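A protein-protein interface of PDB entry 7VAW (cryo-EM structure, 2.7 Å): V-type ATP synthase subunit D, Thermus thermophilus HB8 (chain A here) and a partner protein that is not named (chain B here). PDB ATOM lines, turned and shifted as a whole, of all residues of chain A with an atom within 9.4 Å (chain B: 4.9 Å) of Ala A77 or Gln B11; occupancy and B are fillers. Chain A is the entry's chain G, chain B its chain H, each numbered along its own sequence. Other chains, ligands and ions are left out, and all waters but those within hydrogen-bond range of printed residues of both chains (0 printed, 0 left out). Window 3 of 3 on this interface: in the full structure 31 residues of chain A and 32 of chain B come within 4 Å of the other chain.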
ATOM      1  N   ALA A  60       4.937   5.115  20.253  1.00  0.00           N
ATOM      2  CA  ALA A  60       6.100   5.518  21.034  1.00  0.00           C
ATOM      3  C   ALA A  60       5.793   6.742  21.885  1.00  0.00           C
ATOM      4  O   ALA A  60       6.173   6.801  23.060  1.00  0.00           O
ATOM      5  CB  ALA A  60       7.288   5.789  20.111  1.00  0.00           C
ATOM      6  N   LEU A  64       5.742   7.023  25.927  1.00  0.00           N
ATOM      7  CA  LEU A  64       6.492   8.052  26.640  1.00  0.00           C
ATOM      8  C   LEU A  64       5.593   8.811  27.606  1.00  0.00           C
ATOM      9  O   LEU A  64       5.965   9.052  28.761  1.00  0.00           O
ATOM     10  CB  LEU A  64       7.143   9.014  25.643  1.00  0.00           C
ATOM     11  CG  LEU A  64       8.113  10.080  26.168  1.00  0.00           C
ATOM     12  CD1 LEU A  64       9.119  10.423  25.094  1.00  0.00           C
ATOM     13  CD2 LEU A  64       7.390  11.345  26.611  1.00  0.00           C
ATOM     14  N   ALA A  67       4.643   6.550  30.565  1.00  0.00           N
ATOM     15  CA  ALA A  67       5.777   6.353  31.460  1.00  0.00           C
ATOM     16  C   ALA A  67       6.055   7.604  32.283  1.00  0.00           C
ATOM     17  O   ALA A  67       6.331   7.513  33.484  1.00  0.00           O
ATOM     18  CB  ALA A  67       7.016   5.950  30.662  1.00  0.00           C
ATOM     19  N   GLN A  68       5.984   8.783  31.661  1.00  0.00           N
ATOM     20  CA  GLN A  68       6.218  10.016  32.404  1.00  0.00           C
ATOM     21  C   GLN A  68       5.091  10.325  33.377  1.00  0.00           C
ATOM     22  O   GLN A  68       5.319  11.024  34.370  1.00  0.00           O
ATOM     23  CB  GLN A  68       6.415  11.187  31.442  1.00  0.00           C
ATOM     24  CG  GLN A  68       7.740  11.159  30.704  1.00  0.00           C
ATOM     25  CD  GLN A  68       8.080  12.491  30.072  1.00  0.00           C
ATOM     26  OE1 GLN A  68       7.289  13.433  30.119  1.00  0.00           O
ATOM     27  NE2 GLN A  68       9.264  12.580  29.478  1.00  0.00           N
ATOM     28  N   ASP A  71       5.855   7.538  36.115  1.00  0.00           N
ATOM     29  CA  ASP A  71       7.219   7.566  36.621  1.00  0.00           C
ATOM     30  C   ASP A  71       7.768   8.978  36.490  1.00  0.00           C
ATOM     31  O   ASP A  71       7.425   9.710  35.560  1.00  0.00           O
ATOM     32  CB  ASP A  71       8.118   6.572  35.875  1.00  0.00           C
ATOM     33  CG  ASP A  71       9.486   6.441  36.501  1.00  0.00           C
ATOM     34  OD1 ASP A  71       9.644   6.830  37.676  1.00  0.00           O
ATOM     35  OD2 ASP A  71      10.406   5.948  35.816  1.00  0.00           O
ATOM     36  N   GLY A  72       8.629   9.351  37.432  1.00  0.00           N
ATOM     37  CA  GLY A  72       9.194  10.678  37.461  1.00  0.00           C
ATOM     38  C   GLY A  72      10.122  10.941  36.295  1.00  0.00           C
ATOM     39  O   GLY A  72      10.800  10.038  35.793  1.00  0.00           O
ATOM     40  N   PRO A  73      10.162  12.193  35.833  1.00  0.00           N
ATOM     41  CA  PRO A  73      11.070  12.537  34.727  1.00  0.00           C
ATOM     42  C   PRO A  73      12.527  12.245  35.035  1.00  0.00           C
ATOM     43  O   PRO A  73      13.283  11.869  34.130  1.00  0.00           O
ATOM     44  CB  PRO A  73      10.825  14.039  34.528  1.00  0.00           C
ATOM     45  CG  PRO A  73       9.455  14.276  35.083  1.00  0.00           C
ATOM     46  CD  PRO A  73       9.330  13.336  36.244  1.00  0.00           C
ATOM     47  N   GLU A  74      12.943  12.405  36.292  1.00  0.00           N
ATOM     48  CA  GLU A  74      14.324  12.102  36.655  1.00  0.00           C
ATOM     49  C   GLU A  74      14.627  10.621  36.472  1.00  0.00           C
ATOM     50  O   GLU A  74      15.712  10.258  36.006  1.00  0.00           O
ATOM     51  CB  GLU A  74      14.596  12.536  38.094  1.00  0.00           C
ATOM     52  CG  GLU A  74      14.371  14.017  38.354  1.00  0.00           C
ATOM     53  CD  GLU A  74      15.414  14.899  37.692  1.00  0.00           C
ATOM     54  OE1 GLU A  74      16.487  14.381  37.317  1.00  0.00           O
ATOM     55  OE2 GLU A  74      15.159  16.112  37.547  1.00  0.00           O
ATOM     56  N   VAL A  75      13.678   9.751  36.822  1.00  0.00           N
ATOM     57  CA  VAL A  75      13.915   8.315  36.714  1.00  0.00           C
ATOM     58  C   VAL A  75      14.059   7.896  35.254  1.00  0.00           C
ATOM     59  O   VAL A  75      14.962   7.128  34.904  1.00  0.00           O
ATOM     60  CB  VAL A  75      12.795   7.530  37.419  1.00  0.00           C
ATOM     61  CG1 VAL A  75      13.151   6.054  37.493  1.00  0.00           C
ATOM     62  CG2 VAL A  75      12.547   8.095  38.810  1.00  0.00           C
ATOM     63  N   VAL A  76      13.175   8.382  34.380  1.00  0.00           N
ATOM     64  CA  VAL A  76      13.267   8.011  32.970  1.00  0.00           C
ATOM     65  C   VAL A  76      14.506   8.628  32.330  1.00  0.00           C
ATOM     66  O   VAL A  76      15.142   8.014  31.465  1.00  0.00           O
ATOM     67  CB  VAL A  76      11.977   8.386  32.216  1.00  0.00           C
ATOM     68  CG1 VAL A  76      10.819   7.511  32.680  1.00  0.00           C
ATOM     69  CG2 VAL A  76      11.641   9.852  32.398  1.00  0.00           C
ATOM     70  N   ALA A  77      14.874   9.848  32.737  1.00  0.00           N
ATOM     71  CA  ALA A  77      16.107  10.443  32.233  1.00  0.00           C
ATOM     72  C   ALA A  77      17.325   9.625  32.650  1.00  0.00           C
ATOM     73  O   ALA A  77      18.239   9.397  31.846  1.00  0.00           O
ATOM     74  CB  ALA A  77      16.233  11.885  32.721  1.00  0.00           C
ATOM     75  N   GLY A  78      17.355   9.170  33.905  1.00  0.00           N
ATOM     76  CA  GLY A  78      18.443   8.321  34.353  1.00  0.00           C
ATOM     77  C   GLY A  78      18.466   6.971  33.669  1.00  0.00           C
ATOM     78  O   GLY A  78      19.538   6.409  33.436  1.00  0.00           O
ATOM     79  N   ALA A  79      17.291   6.423  33.355  1.00  0.00           N
ATOM     80  CA  ALA A  79      17.235   5.184  32.586  1.00  0.00           C
ATOM     81  C   ALA A  79      17.785   5.386  31.181  1.00  0.00           C
ATOM     82  O   ALA A  79      18.501   4.524  30.657  1.00  0.00           O
ATOM     83  CB  ALA A  79      15.800   4.661  32.531  1.00  0.00           C
ATOM     84  N   ALA A  80      17.456   6.517  30.554  1.00  0.00           N
ATOM     85  CA  ALA A  80      18.015   6.835  29.244  1.00  0.00           C
ATOM     86  C   ALA A  80      19.528   6.990  29.319  1.00  0.00           C
ATOM     87  O   ALA A  80      20.250   6.582  28.402  1.00  0.00           O
ATOM     88  CB  ALA A  80      17.373   8.106  28.694  1.00  0.00           C
ATOM     89  N   LEU A  81      20.022   7.601  30.397  1.00  0.00           N
ATOM     90  CA  LEU A  81      21.466   7.706  30.593  1.00  0.00           C
ATOM     91  C   LEU A  81      22.102   6.332  30.773  1.00  0.00           C
ATOM     92  O   LEU A  81      23.190   6.069  30.246  1.00  0.00           O
ATOM     93  CB  LEU A  81      21.767   8.596  31.797  1.00  0.00           C
ATOM     94  CG  LEU A  81      23.235   8.693  32.223  1.00  0.00           C
ATOM     95  CD1 LEU A  81      24.056   9.432  31.179  1.00  0.00           C
ATOM     96  CD2 LEU A  81      23.364   9.357  33.588  1.00  0.00           C
ATOM     97  N   GLY A  82      21.437   5.445  31.516  1.00  0.00           N
ATOM     98  CA  GLY A  82      22.049   4.175  31.872  1.00  0.00           C
ATOM     99  C   GLY A  82      22.318   3.278  30.679  1.00  0.00           C
ATOM    100  O   GLY A  82      23.362   2.624  30.610  1.00  0.00           O
ATOM    101  N   VAL A  83      21.387   3.226  29.736  1.00  0.00           N
ATOM    102  CA  VAL A  83      21.577   2.370  28.560  1.00  0.00           C
ATOM    103  C   VAL A  83      22.731   2.910  27.720  1.00  0.00           C
ATOM    104  O   VAL A  83      22.771   4.120  27.426  1.00  0.00           O
ATOM    105  CB  VAL A  83      20.278   2.276  27.745  1.00  0.00           C
ATOM    106  CG1 VAL A  83      19.837   3.638  27.231  1.00  0.00           C
ATOM    107  CG2 VAL A  83      20.458   1.319  26.578  1.00  0.00           C
ATOM    108  N   PRO A 120      11.161   0.509  36.079  1.00  0.00           N
ATOM    109  CA  PRO A 120       9.764   0.879  36.344  1.00  0.00           C
ATOM    110  C   PRO A 120       8.795   0.145  35.429  1.00  0.00           C
ATOM    111  O   PRO A 120       9.173  -0.557  34.489  1.00  0.00           O
ATOM    112  CB  PRO A 120       9.743   2.390  36.092  1.00  0.00           C
ATOM    113  CG  PRO A 120      11.132   2.826  36.389  1.00  0.00           C
ATOM    114  CD  PRO A 120      12.025   1.698  35.950  1.00  0.00           C
ATOM    115  N   THR A 123       8.745   1.271  31.628  1.00  0.00           N
ATOM    116  CA  THR A 123      10.019   1.555  30.975  1.00  0.00           C
ATOM    117  C   THR A 123      10.319   0.538  29.880  1.00  0.00           C
ATOM    118  O   THR A 123      10.827   0.900  28.813  1.00  0.00           O
ATOM    119  CB  THR A 123      11.143   1.585  32.008  1.00  0.00           C
ATOM    120  OG1 THR A 123      10.841   2.564  33.010  1.00  0.00           O
ATOM    121  CG2 THR A 123      12.468   1.939  31.349  1.00  0.00           C
ATOM    122  N   ALA A 126       8.040   1.347  26.817  1.00  0.00           N
ATOM    123  CA  ALA A 126       8.556   2.498  26.088  1.00  0.00           C
ATOM    124  C   ALA A 126       9.838   2.147  25.344  1.00  0.00           C
ATOM    125  O   ALA A 126      10.041   2.582  24.206  1.00  0.00           O
ATOM    126  CB  ALA A 126       8.790   3.666  27.046  1.00  0.00           C
ATOM    127  N   SER A 127      10.708   1.350  25.969  1.00  0.00           N
ATOM    128  CA  SER A 127      11.965   0.972  25.330  1.00  0.00           C
ATOM    129  C   SER A 127      11.718   0.172  24.059  1.00  0.00           C
ATOM    130  O   SER A 127      12.288   0.473  23.003  1.00  0.00           O
ATOM    131  CB  SER A 127      12.828   0.174  26.309  1.00  0.00           C
ATOM    132  OG  SER A 127      13.146   0.947  27.452  1.00  0.00           O
ATOM    133  N   PHE A 130      10.063   2.399  21.318  1.00  0.00           N
ATOM    134  CA  PHE A 130      10.995   3.311  20.669  1.00  0.00           C
ATOM    135  C   PHE A 130      12.029   2.566  19.838  1.00  0.00           C
ATOM    136  O   PHE A 130      12.478   3.081  18.813  1.00  0.00           O
ATOM    137  CB  PHE A 130      11.675   4.198  21.707  1.00  0.00           C
ATOM    138  CG  PHE A 130      10.974   5.505  21.929  1.00  0.00           C
ATOM    139  CD1 PHE A 130      11.294   6.614  21.165  1.00  0.00           C
ATOM    140  CD2 PHE A 130       9.983   5.619  22.887  1.00  0.00           C
ATOM    141  CE1 PHE A 130      10.647   7.817  21.362  1.00  0.00           C
ATOM    142  CE2 PHE A 130       9.332   6.819  23.087  1.00  0.00           C
ATOM    143  CZ  PHE A 130       9.664   7.920  22.324  1.00  0.00           C
ATOM    144  N   PRO B   7      12.342  18.493  23.212  1.00  0.00           N
ATOM    145  CA  PRO B   7      13.091  17.770  24.254  1.00  0.00           C
ATOM    146  C   PRO B   7      12.415  16.491  24.716  1.00  0.00           C
ATOM    147  O   PRO B   7      13.109  15.559  25.141  1.00  0.00           O
ATOM    148  CB  PRO B   7      13.192  18.799  25.390  1.00  0.00           C
ATOM    149  CG  PRO B   7      12.105  19.792  25.114  1.00  0.00           C
ATOM    150  CD  PRO B   7      12.031  19.871  23.625  1.00  0.00           C
ATOM    151  N   GLU B   8      11.086  16.414  24.645  1.00  0.00           N
ATOM    152  CA  GLU B   8      10.397  15.173  24.986  1.00  0.00           C
ATOM    153  C   GLU B   8      10.791  14.047  24.034  1.00  0.00           C
ATOM    154  O   GLU B   8      11.128  12.939  24.468  1.00  0.00           O
ATOM    155  CB  GLU B   8       8.885  15.394  24.967  1.00  0.00           C
ATOM    156  CG  GLU B   8       8.380  16.302  26.077  1.00  0.00           C
ATOM    157  CD  GLU B   8       6.933  16.715  25.885  1.00  0.00           C
ATOM    158  OE1 GLU B   8       6.185  15.977  25.209  1.00  0.00           O
ATOM    159  OE2 GLU B   8       6.543  17.779  26.411  1.00  0.00           O
ATOM    160  N   THR B   9      10.763  14.319  22.726  1.00  0.00           N
ATOM    161  CA  THR B   9      11.131  13.296  21.751  1.00  0.00           C
ATOM    162  C   THR B   9      12.611  12.949  21.846  1.00  0.00           C
ATOM    163  O   THR B   9      12.994  11.785  21.678  1.00  0.00           O
ATOM    164  CB  THR B   9      10.777  13.763  20.339  1.00  0.00           C
ATOM    165  OG1 THR B   9       9.403  14.165  20.299  1.00  0.00           O
ATOM    166  CG2 THR B   9      10.994  12.640  19.333  1.00  0.00           C
ATOM    167  N   ALA B  10      13.460  13.944  22.110  1.00  0.00           N
ATOM    168  CA  ALA B  10      14.882  13.668  22.288  1.00  0.00           C
ATOM    169  C   ALA B  10      15.120  12.775  23.498  1.00  0.00           C
ATOM    170  O   ALA B  10      15.941  11.851  23.446  1.00  0.00           O
ATOM    171  CB  ALA B  10      15.660  14.976  22.418  1.00  0.00           C
ATOM    172  N   GLN B  11      14.408  13.032  24.598  1.00  0.00           N
ATOM    173  CA  GLN B  11      14.509  12.164  25.766  1.00  0.00           C
ATOM    174  C   GLN B  11      14.009  10.759  25.455  1.00  0.00           C
ATOM    175  O   GLN B  11      14.603   9.769  25.892  1.00  0.00           O
ATOM    176  CB  GLN B  11      13.728  12.761  26.937  1.00  0.00           C
ATOM    177  CG  GLN B  11      14.439  13.906  27.641  1.00  0.00           C
ATOM    178  CD  GLN B  11      15.551  13.435  28.560  1.00  0.00           C
ATOM    179  OE1 GLN B  11      15.781  12.236  28.717  1.00  0.00           O
ATOM    180  NE2 GLN B  11      16.248  14.381  29.176  1.00  0.00           N
ATOM    181  N   GLY B  12      12.908  10.656  24.707  1.00  0.00           N
ATOM    182  CA  GLY B  12      12.394   9.344  24.348  1.00  0.00           C
ATOM    183  C   GLY B  12      13.349   8.560  23.469  1.00  0.00           C
ATOM    184  O   GLY B  12      13.445   7.336  23.576  1.00  0.00           O
ATOM    185  N   PHE B  13      14.058   9.253  22.579  1.00  0.00           N
ATOM    186  CA  PHE B  13      15.039   8.575  21.739  1.00  0.00           C
ATOM    187  C   PHE B  13      16.282   8.197  22.535  1.00  0.00           C
ATOM    188  O   PHE B  13      16.869   7.133  22.308  1.00  0.00           O
ATOM    189  CB  PHE B  13      15.399   9.448  20.540  1.00  0.00           C
ATOM    190  CG  PHE B  13      14.569   9.164  19.325  1.00  0.00           C
ATOM    191  CD1 PHE B  13      14.775   8.010  18.589  1.00  0.00           C
ATOM    192  CD2 PHE B  13      13.572  10.038  18.927  1.00  0.00           C
ATOM    193  CE1 PHE B  13      14.010   7.737  17.473  1.00  0.00           C
ATOM    194  CE2 PHE B  13      12.803   9.772  17.812  1.00  0.00           C
ATOM    195  CZ  PHE B  13      13.025   8.621  17.084  1.00  0.00           C
ATOM    196  N   ARG B  14      16.701   9.055  23.470  1.00  0.00           N
ATOM    197  CA  ARG B  14      17.778   8.679  24.378  1.00  0.00           C
ATOM    198  C   ARG B  14      17.383   7.485  25.235  1.00  0.00           C
ATOM    199  O   ARG B  14      18.247   6.709  25.660  1.00  0.00           O
ATOM    200  CB  ARG B  14      18.162   9.865  25.262  1.00  0.00           C
ATOM    201  CG  ARG B  14      18.868  10.986  24.526  1.00  0.00           C
ATOM    202  CD  ARG B  14      20.308  10.617  24.212  1.00  0.00           C
ATOM    203  NE  ARG B  14      21.165  10.713  25.387  1.00  0.00           N
ATOM    204  CZ  ARG B  14      21.964  11.739  25.648  1.00  0.00           C
ATOM    205  NH1 ARG B  14      22.035  12.784  24.839  1.00  0.00           N
ATOM    206  NH2 ARG B  14      22.708  11.718  26.750  1.00  0.00           N
ATOM    207  N   LEU B  15      16.083   7.328  25.500  1.00  0.00           N
ATOM    208  CA  LEU B  15      15.594   6.175  26.246  1.00  0.00           C
ATOM    209  C   LEU B  15      15.892   4.872  25.518  1.00  0.00           C
ATOM    210  O   LEU B  15      16.126   3.842  26.160  1.00  0.00           O
ATOM    211  CB  LEU B  15      14.093   6.336  26.503  1.00  0.00           C
ATOM    212  CG  LEU B  15      13.331   5.322  27.354  1.00  0.00           C
ATOM    213  CD1 LEU B  15      12.248   6.028  28.145  1.00  0.00           C
ATOM    214  CD2 LEU B  15      12.712   4.259  26.474  1.00  0.00           C
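O of Ala A80 sits close to O of Arg B14, 3.4 Å away.
O of Thr A123 is in hydrogen-bond range of OG of Ser A127, 2.7 Å away.
Among the printed residues, pairs that only touch across the chains: Leu A64 with Glu B8 (3.3 Å), Leu A64 with Gly B12 (3.5 Å), Ala A77 with Gln B11 (3.96 Å), Ala A80 with Leu B15 (3.5 Å), Val A83 with Arg B14 (3.8 Å), Val A83 with Leu B15 (3.9 Å), Ala A126 with Leu B15 (3.7 Å), Ser A127 with Leu B15 (3.5 Å), Phe A130 with Gly B12 (3.3 Å) and Phe A130 with Phe B13 (3.9 Å).
Pro A73 touches none of the printed residues of chain B.
Ala A77 touches just one residue of chain B: Gln B11 (3.96 Å).
Thr A123 touches none of the printed residues of chain B.
Printed residues of chain B within 4 Å of Ala A126: Leu B15 (3.7 Å).
No residue of chain A comes within 4 Å of Ala B10.
Of chain A, only Ala A77 comes within 4 Å of Gln B11.
Of the printed residues of chain A, Arg B14 touches Ala A80 (3.4 Å) and Val A83 (3.8 Å).
The nearest printed residue of chain B that does not touch Leu A64 is Thr B9 (4.8 Å).
Of the 9 printed residues of chain B, 6 touch a printed residue of chain A.
Hydrophobic or aromatic side chains of chain B that line the printed part of chain A: Leu B15.
Of the 22 printed residues of chain A, 7 touch a printed residue of chain B.
Along chain A the printed residues that touch a printed residue of chain B span positions 64 to 130.
Among the printed residues, no Asp or Glu carboxylate lies within 4 Å of a Lys or Arg side-chain nitrogen of the other chain.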
